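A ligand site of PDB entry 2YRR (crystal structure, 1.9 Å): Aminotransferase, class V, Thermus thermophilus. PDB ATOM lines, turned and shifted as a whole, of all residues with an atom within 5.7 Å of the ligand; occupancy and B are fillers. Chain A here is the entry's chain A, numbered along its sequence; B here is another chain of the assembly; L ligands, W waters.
The side-chain hydroxyl of Ser 60 lies close to the backbone NH of Ser 62 (3.4 Å). The side-chain hydroxyl (OH) of Tyr 214 of chain B sits at hydrogen-bond distance from the backbone NH (N) of Ser 60, at 3.0 Å. The guanidinium group (NH1) of Arg 88 is in hydrogen-bond range of the side-chain hydroxyl (OH) of Tyr 229 of chain B (3.3 Å). The side-chain hydroxyl of Ser 62 sits at hydrogen-bond distance from the guanidinium group of Arg 88. The side-chain carboxylate (OD1) of Asp 160 sits at hydrogen-bond distance from the backbone NH (N) of Val 162 (3.0 Å). The backbone carbonyl oxygen (O) of Gly 133 lies close to the side-chain hydroxyl (OG1) of Thr 163, 3.0 Å away. The side-chain hydroxyl (OG) of Ser 60 is in hydrogen-bond range of a ring nitrogen (ND1) of His 231 of chain B (3.2 Å). The backbone NH of Phe 85 is in hydrogen-bond range of the side-chain carboxylate of Glu 134.
The side-chain hydroxyl of Ser 62 sits at hydrogen-bond distance from an oxygen (O5) of the ligand. OG of Ser 60 is in hydrogen-bond range of O5 of the ligand (2.7 Å). N of Ser 62 lies within hydrogen-bond range of O5 of the ligand, 2.7 Å away. An oxygen (O3) of the ligand lies within hydrogen-bond range of the backbone NH (N) of Gly 61 (2.9 Å). The side-chain hydroxyl (OG1) of Thr 232 of chain B sits at hydrogen-bond distance from an oxygen (O4) of the ligand (2.6 Å). The side-chain amino group of Lys 186 is covalently linked to a carbon (C5) of the ligand (1.5 Å). The side-chain carboxylate (OD2) of Asp 160 is in hydrogen-bond range of a nitrogen (N1) of the ligand, 2.5 Å away. O1 of the ligand sits at hydrogen-bond distance from OG1 of Thr 135 (2.5 Å). NE2 of Gln 185 is in hydrogen-bond range of O3 of the ligand (2.7 Å). The side-chain hydroxyl (OH) of Tyr 229 of chain B is in hydrogen-bond range of an oxygen (O4) of the ligand (3.0 Å). An oxygen (O4) of the ligand is in hydrogen-bond range of the backbone NH (N) of Thr 232 of chain B, at 2.9 Å.
Merely in contact with the ligand: Val 162 (3.3 Å), Phe 85 (3.5 Å), Gly 133 (3.6 Å), His 231 of chain B (3.6 Å), Val 131 (3.9 Å), Arg 88 (3.9 Å) and Thr 163 (3.98 Å). Hydrophobic or aromatic side chains that line the ligand: Phe 85, Val 131, Val 162 and His 231 of chain B. 16 residues have an atom within 4 Å of the ligand: Ser 60, Gly 61, Ser 62, Phe 85, Arg 88, Val 131, Gly 133, Thr 135, Asp 160, Val 162, Thr 163, Gln 185, Lys 186, Tyr 229 of chain B, His 231 of chain B and Thr 232 of chain B.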
ATOM      1  N   PRO A   6     -15.696 -20.346 -35.190  1.00  0.00           N
ATOM      2  CA  PRO A   6     -15.995 -21.265 -34.095  1.00  0.00           C
ATOM      3  C   PRO A   6     -17.085 -20.669 -33.201  1.00  0.00           C
ATOM      4  O   PRO A   6     -16.927 -20.557 -31.984  1.00  0.00           O
ATOM      5  CB  PRO A   6     -14.660 -21.409 -33.381  1.00  0.00           C
ATOM      6  CG  PRO A   6     -14.029 -20.087 -33.596  1.00  0.00           C
ATOM      7  CD  PRO A   6     -14.330 -19.794 -35.047  1.00  0.00           C
ATOM      8  N   SER A  60     -26.108 -13.826 -24.416  1.00  0.00           N
ATOM      9  CA  SER A  60     -25.076 -14.665 -25.018  1.00  0.00           C
ATOM     10  C   SER A  60     -24.487 -15.643 -23.996  1.00  0.00           C
ATOM     11  O   SER A  60     -24.821 -15.590 -22.814  1.00  0.00           O
ATOM     12  CB  SER A  60     -23.949 -13.803 -25.584  1.00  0.00           C
ATOM     13  OG  SER A  60     -23.154 -13.272 -24.535  1.00  0.00           O
ATOM     14  N   GLY A  61     -23.605 -16.523 -24.454  1.00  0.00           N
ATOM     15  CA  GLY A  61     -22.991 -17.487 -23.550  1.00  0.00           C
ATOM     16  C   GLY A  61     -22.297 -16.840 -22.367  1.00  0.00           C
ATOM     17  O   GLY A  61     -22.275 -17.401 -21.264  1.00  0.00           O
ATOM     18  N   SER A  62     -21.736 -15.665 -22.580  1.00  0.00           N
ATOM     19  CA  SER A  62     -21.032 -14.966 -21.515  1.00  0.00           C
ATOM     20  C   SER A  62     -21.954 -14.665 -20.329  1.00  0.00           C
ATOM     21  O   SER A  62     -21.495 -14.594 -19.176  1.00  0.00           O
ATOM     22  CB  SER A  62     -20.414 -13.680 -22.062  1.00  0.00           C
ATOM     23  OG  SER A  62     -19.323 -13.997 -22.902  1.00  0.00           O
ATOM     24  N   LEU A  63     -23.234 -14.488 -20.606  1.00  0.00           N
ATOM     25  CA  LEU A  63     -24.204 -14.235 -19.551  1.00  0.00           C
ATOM     26  C   LEU A  63     -24.311 -15.514 -18.734  1.00  0.00           C
ATOM     27  O   LEU A  63     -24.369 -15.480 -17.501  1.00  0.00           O
ATOM     28  CB  LEU A  63     -25.576 -13.894 -20.147  1.00  0.00           C
ATOM     29  CG  LEU A  63     -26.714 -13.669 -19.150  1.00  0.00           C
ATOM     30  CD1 LEU A  63     -26.347 -12.551 -18.190  1.00  0.00           C
ATOM     31  CD2 LEU A  63     -28.013 -13.340 -19.892  1.00  0.00           C
ATOM     32  N   MET A  65     -22.027 -17.669 -18.377  1.00  0.00           N
ATOM     33  CA  MET A  65     -20.769 -17.770 -17.651  1.00  0.00           C
ATOM     34  C   MET A  65     -20.807 -16.944 -16.371  1.00  0.00           C
ATOM     35  O   MET A  65     -20.463 -17.437 -15.293  1.00  0.00           O
ATOM     36  CB  MET A  65     -19.615 -17.296 -18.534  1.00  0.00           C
ATOM     37  CG  MET A  65     -18.242 -17.432 -17.899  1.00  0.00           C
ATOM     38  SD  MET A  65     -16.965 -16.564 -18.821  1.00  0.00           S
ATOM     39  CE  MET A  65     -16.466 -17.898 -19.942  1.00  0.00           C
ATOM     40  N   PHE A  85     -11.024 -17.610 -22.934  1.00  0.00           N
ATOM     41  CA  PHE A  85     -12.268 -17.782 -22.207  1.00  0.00           C
ATOM     42  C   PHE A  85     -12.151 -18.156 -20.726  1.00  0.00           C
ATOM     43  O   PHE A  85     -13.010 -17.796 -19.933  1.00  0.00           O
ATOM     44  CB  PHE A  85     -13.171 -18.737 -22.983  1.00  0.00           C
ATOM     45  CG  PHE A  85     -13.531 -18.211 -24.346  1.00  0.00           C
ATOM     46  CD1 PHE A  85     -12.883 -18.671 -25.480  1.00  0.00           C
ATOM     47  CD2 PHE A  85     -14.478 -17.190 -24.476  1.00  0.00           C
ATOM     48  CE1 PHE A  85     -13.157 -18.105 -26.729  1.00  0.00           C
ATOM     49  CE2 PHE A  85     -14.760 -16.629 -25.724  1.00  0.00           C
ATOM     50  CZ  PHE A  85     -14.102 -17.083 -26.850  1.00  0.00           C
ATOM     51  N   ARG A  88     -11.522 -15.035 -19.068  1.00  0.00           N
ATOM     52  CA  ARG A  88     -12.735 -14.257 -18.887  1.00  0.00           C
ATOM     53  C   ARG A  88     -13.389 -14.693 -17.572  1.00  0.00           C
ATOM     54  O   ARG A  88     -13.934 -13.878 -16.837  1.00  0.00           O
ATOM     55  CB  ARG A  88     -13.714 -14.481 -20.053  1.00  0.00           C
ATOM     56  CG  ARG A  88     -15.000 -13.676 -19.942  1.00  0.00           C
ATOM     57  CD  ARG A  88     -15.843 -13.751 -21.194  1.00  0.00           C
ATOM     58  NE  ARG A  88     -15.145 -13.185 -22.353  1.00  0.00           N
ATOM     59  CZ  ARG A  88     -15.561 -13.279 -23.604  1.00  0.00           C
ATOM     60  NH1 ARG A  88     -16.697 -13.905 -23.898  1.00  0.00           N
ATOM     61  NH2 ARG A  88     -14.830 -12.752 -24.583  1.00  0.00           N
ATOM     62  N   VAL A 131     -12.723 -24.519 -18.321  1.00  0.00           N
ATOM     63  CA  VAL A 131     -13.355 -24.395 -19.616  1.00  0.00           C
ATOM     64  C   VAL A 131     -13.114 -25.744 -20.289  1.00  0.00           C
ATOM     65  O   VAL A 131     -11.961 -26.134 -20.504  1.00  0.00           O
ATOM     66  CB  VAL A 131     -12.717 -23.294 -20.472  1.00  0.00           C
ATOM     67  CG1 VAL A 131     -13.208 -23.415 -21.910  1.00  0.00           C
ATOM     68  CG2 VAL A 131     -13.075 -21.921 -19.910  1.00  0.00           C
ATOM     69  N   GLY A 133     -13.661 -26.945 -23.474  1.00  0.00           N
ATOM     70  CA  GLY A 133     -12.914 -26.804 -24.706  1.00  0.00           C
ATOM     71  C   GLY A 133     -12.525 -25.350 -24.864  1.00  0.00           C
ATOM     72  O   GLY A 133     -13.381 -24.483 -25.022  1.00  0.00           O
ATOM     73  N   GLU A 134     -11.219 -25.068 -24.784  1.00  0.00           N
ATOM     74  CA  GLU A 134     -10.736 -23.697 -24.903  1.00  0.00           C
ATOM     75  C   GLU A 134     -10.660 -23.288 -26.361  1.00  0.00           C
ATOM     76  O   GLU A 134      -9.688 -23.587 -27.068  1.00  0.00           O
ATOM     77  CB  GLU A 134      -9.370 -23.561 -24.213  1.00  0.00           C
ATOM     78  CG  GLU A 134      -8.754 -22.173 -24.297  1.00  0.00           C
ATOM     79  CD  GLU A 134      -9.705 -21.073 -23.840  1.00  0.00           C
ATOM     80  OE1 GLU A 134     -10.163 -21.117 -22.679  1.00  0.00           O
ATOM     81  OE2 GLU A 134      -9.982 -20.161 -24.641  1.00  0.00           O
ATOM     82  N   THR A 135     -11.709 -22.597 -26.808  1.00  0.00           N
ATOM     83  CA  THR A 135     -11.839 -22.153 -28.189  1.00  0.00           C
ATOM     84  C   THR A 135     -10.725 -21.266 -28.733  1.00  0.00           C
ATOM     85  O   THR A 135     -10.505 -21.237 -29.940  1.00  0.00           O
ATOM     86  CB  THR A 135     -13.164 -21.392 -28.373  1.00  0.00           C
ATOM     87  OG1 THR A 135     -14.167 -21.989 -27.542  1.00  0.00           O
ATOM     88  CG2 THR A 135     -13.622 -21.454 -29.812  1.00  0.00           C
ATOM     89  N   ASP A 160     -17.333 -24.567 -18.389  1.00  0.00           N
ATOM     90  CA  ASP A 160     -17.754 -23.910 -19.615  1.00  0.00           C
ATOM     91  C   ASP A 160     -17.822 -25.021 -20.663  1.00  0.00           C
ATOM     92  O   ASP A 160     -16.793 -25.546 -21.070  1.00  0.00           O
ATOM     93  CB  ASP A 160     -16.695 -22.876 -20.006  1.00  0.00           C
ATOM     94  CG  ASP A 160     -16.968 -22.218 -21.343  1.00  0.00           C
ATOM     95  OD1 ASP A 160     -17.422 -22.909 -22.283  1.00  0.00           O
ATOM     96  OD2 ASP A 160     -16.681 -21.009 -21.455  1.00  0.00           O
ATOM     97  N   VAL A 162     -19.229 -24.727 -23.770  1.00  0.00           N
ATOM     98  CA  VAL A 162     -19.539 -24.146 -25.074  1.00  0.00           C
ATOM     99  C   VAL A 162     -19.094 -24.948 -26.301  1.00  0.00           C
ATOM    100  O   VAL A 162     -19.861 -25.100 -27.257  1.00  0.00           O
ATOM    101  CB  VAL A 162     -18.947 -22.736 -25.196  1.00  0.00           C
ATOM    102  CG1 VAL A 162     -19.068 -22.234 -26.623  1.00  0.00           C
ATOM    103  CG2 VAL A 162     -19.678 -21.784 -24.251  1.00  0.00           C
ATOM    104  N   THR A 163     -17.861 -25.445 -26.290  1.00  0.00           N
ATOM    105  CA  THR A 163     -17.353 -26.184 -27.430  1.00  0.00           C
ATOM    106  C   THR A 163     -17.536 -27.696 -27.369  1.00  0.00           C
ATOM    107  O   THR A 163     -17.007 -28.417 -28.209  1.00  0.00           O
ATOM    108  CB  THR A 163     -15.852 -25.918 -27.631  1.00  0.00           C
ATOM    109  OG1 THR A 163     -15.126 -26.404 -26.504  1.00  0.00           O
ATOM    110  CG2 THR A 163     -15.588 -24.442 -27.776  1.00  0.00           C
ATOM    111  N   PHE A 181     -22.683 -24.533 -18.800  1.00  0.00           N
ATOM    112  CA  PHE A 181     -23.381 -23.594 -19.656  1.00  0.00           C
ATOM    113  C   PHE A 181     -22.804 -23.571 -21.063  1.00  0.00           C
ATOM    114  O   PHE A 181     -21.707 -24.071 -21.321  1.00  0.00           O
ATOM    115  CB  PHE A 181     -23.276 -22.194 -19.062  1.00  0.00           C
ATOM    116  CG  PHE A 181     -21.913 -21.575 -19.208  1.00  0.00           C
ATOM    117  CD1 PHE A 181     -21.597 -20.814 -20.337  1.00  0.00           C
ATOM    118  CD2 PHE A 181     -20.938 -21.779 -18.239  1.00  0.00           C
ATOM    119  CE1 PHE A 181     -20.336 -20.265 -20.491  1.00  0.00           C
ATOM    120  CE2 PHE A 181     -19.666 -21.225 -18.384  1.00  0.00           C
ATOM    121  CZ  PHE A 181     -19.367 -20.475 -19.509  1.00  0.00           C
ATOM    122  N   GLY A 183     -23.806 -21.468 -25.250  1.00  0.00           N
ATOM    123  CA  GLY A 183     -24.512 -20.411 -25.949  1.00  0.00           C
ATOM    124  C   GLY A 183     -25.311 -21.089 -27.038  1.00  0.00           C
ATOM    125  O   GLY A 183     -24.926 -22.155 -27.512  1.00  0.00           O
ATOM    126  N   GLN A 185     -25.654 -20.285 -30.136  1.00  0.00           N
ATOM    127  CA  GLN A 185     -24.970 -20.269 -31.430  1.00  0.00           C
ATOM    128  C   GLN A 185     -23.726 -21.137 -31.590  1.00  0.00           C
ATOM    129  O   GLN A 185     -23.070 -21.085 -32.626  1.00  0.00           O
ATOM    130  CB  GLN A 185     -24.599 -18.825 -31.797  1.00  0.00           C
ATOM    131  CG  GLN A 185     -23.315 -18.305 -31.147  1.00  0.00           C
ATOM    132  CD  GLN A 185     -23.467 -17.937 -29.673  1.00  0.00           C
ATOM    133  OE1 GLN A 185     -24.473 -18.243 -29.033  1.00  0.00           O
ATOM    134  NE2 GLN A 185     -22.455 -17.268 -29.144  1.00  0.00           N
ATOM    135  N   LYS A 186     -23.398 -21.929 -30.582  1.00  0.00           N
ATOM    136  CA  LYS A 186     -22.202 -22.762 -30.684  1.00  0.00           C
ATOM    137  C   LYS A 186     -22.498 -24.121 -31.326  1.00  0.00           C
ATOM    138  O   LYS A 186     -22.948 -24.185 -32.471  1.00  0.00           O
ATOM    139  CB  LYS A 186     -21.578 -22.911 -29.284  1.00  0.00           C
ATOM    140  CG  LYS A 186     -21.174 -21.546 -28.694  1.00  0.00           C
ATOM    141  CD  LYS A 186     -20.148 -20.842 -29.588  1.00  0.00           C
ATOM    142  CE  LYS A 186     -19.680 -19.479 -29.050  1.00  0.00           C
ATOM    143  NZ  LYS A 186     -18.268 -19.473 -28.667  1.00  0.00           N
ATOM    144  N   TYR B 214     -21.266  -8.479 -18.063  1.00  0.00           N
ATOM    145  CA  TYR B 214     -22.173  -8.460 -19.197  1.00  0.00           C
ATOM    146  C   TYR B 214     -22.797  -7.084 -19.432  1.00  0.00           C
ATOM    147  O   TYR B 214     -22.946  -6.658 -20.573  1.00  0.00           O
ATOM    148  CB  TYR B 214     -23.277  -9.489 -18.982  1.00  0.00           C
ATOM    149  CG  TYR B 214     -24.015  -9.856 -20.246  1.00  0.00           C
ATOM    150  CD1 TYR B 214     -23.404 -10.606 -21.252  1.00  0.00           C
ATOM    151  CD2 TYR B 214     -25.342  -9.462 -20.437  1.00  0.00           C
ATOM    152  CE1 TYR B 214     -24.084 -10.952 -22.416  1.00  0.00           C
ATOM    153  CE2 TYR B 214     -26.035  -9.804 -21.598  1.00  0.00           C
ATOM    154  CZ  TYR B 214     -25.405 -10.556 -22.578  1.00  0.00           C
ATOM    155  OH  TYR B 214     -26.101 -10.902 -23.708  1.00  0.00           O
ATOM    156  N   TYR B 229     -14.424  -6.848 -29.814  1.00  0.00           N
ATOM    157  CA  TYR B 229     -15.202  -7.984 -29.337  1.00  0.00           C
ATOM    158  C   TYR B 229     -15.522  -7.869 -27.856  1.00  0.00           C
ATOM    159  O   TYR B 229     -14.637  -7.725 -27.013  1.00  0.00           O
ATOM    160  CB  TYR B 229     -14.441  -9.306 -29.581  1.00  0.00           C
ATOM    161  CG  TYR B 229     -15.109 -10.534 -28.966  1.00  0.00           C
ATOM    162  CD1 TYR B 229     -16.429 -10.872 -29.275  1.00  0.00           C
ATOM    163  CD2 TYR B 229     -14.429 -11.343 -28.055  1.00  0.00           C
ATOM    164  CE1 TYR B 229     -17.058 -11.973 -28.696  1.00  0.00           C
ATOM    165  CE2 TYR B 229     -15.045 -12.460 -27.468  1.00  0.00           C
ATOM    166  CZ  TYR B 229     -16.362 -12.770 -27.788  1.00  0.00           C
ATOM    167  OH  TYR B 229     -16.981 -13.855 -27.172  1.00  0.00           O
ATOM    168  N   HIS B 231     -18.831  -9.597 -26.696  1.00  0.00           N
ATOM    169  CA  HIS B 231     -19.371 -10.949 -26.710  1.00  0.00           C
ATOM    170  C   HIS B 231     -20.240 -11.055 -27.956  1.00  0.00           C
ATOM    171  O   HIS B 231     -20.574 -10.037 -28.570  1.00  0.00           O
ATOM    172  CB  HIS B 231     -20.193 -11.219 -25.445  1.00  0.00           C
ATOM    173  CG  HIS B 231     -21.427 -10.365 -25.336  1.00  0.00           C
ATOM    174  ND1 HIS B 231     -22.531 -10.555 -26.134  1.00  0.00           N
ATOM    175  CD2 HIS B 231     -21.713  -9.326 -24.523  1.00  0.00           C
ATOM    176  CE1 HIS B 231     -23.456  -9.659 -25.811  1.00  0.00           C
ATOM    177  NE2 HIS B 231     -22.978  -8.904 -24.839  1.00  0.00           N
ATOM    178  N   THR B 232     -20.594 -12.278 -28.330  1.00  0.00           N
ATOM    179  CA  THR B 232     -21.408 -12.495 -29.518  1.00  0.00           C
ATOM    180  C   THR B 232     -22.793 -11.872 -29.365  1.00  0.00           C
ATOM    181  O   THR B 232     -23.461 -12.053 -28.349  1.00  0.00           O
ATOM    182  CB  THR B 232     -21.572 -14.007 -29.797  1.00  0.00           C
ATOM    183  OG1 THR B 232     -20.276 -14.613 -29.852  1.00  0.00           O
ATOM    184  CG2 THR B 232     -22.260 -14.224 -31.141  1.00  0.00           C
HETATM  185  N1  LIG L   1     -16.732 -19.688 -23.611  1.00  0.00           N
HETATM  186  C1  LIG L   1     -16.277 -20.344 -24.726  1.00  0.00           C
HETATM  187  C2  LIG L   1     -15.304 -21.523 -24.540  1.00  0.00           C
HETATM  188  C3  LIG L   1     -16.683 -19.931 -25.991  1.00  0.00           C
HETATM  189  O1  LIG L   1     -16.216 -20.564 -27.141  1.00  0.00           O
HETATM  190  C4  LIG L   1     -17.549 -18.865 -26.120  1.00  0.00           C
HETATM  191  C5  LIG L   1     -18.018 -18.507 -27.553  1.00  0.00           C
HETATM  192  C6  LIG L   1     -18.003 -18.211 -24.953  1.00  0.00           C
HETATM  193  C7  LIG L   1     -17.590 -18.630 -23.730  1.00  0.00           C
HETATM  194  C8  LIG L   1     -18.935 -16.983 -24.926  1.00  0.00           C
HETATM  195  O2  LIG L   1     -20.068 -16.901 -25.715  1.00  0.00           O
HETATM  196  P1  LIG L   1     -20.585 -15.481 -26.208  1.00  0.00           P
HETATM  197  O3  LIG L   1     -21.862 -16.211 -26.775  1.00  0.00           O
HETATM  198  O4  LIG L   1     -19.806 -14.863 -27.294  1.00  0.00           O
HETATM  199  O5  LIG L   1     -20.908 -14.702 -25.013  1.00  0.00           O
HETATM  200  O   HOH W   1     -16.638 -16.170 -29.639  1.00  0.00           O
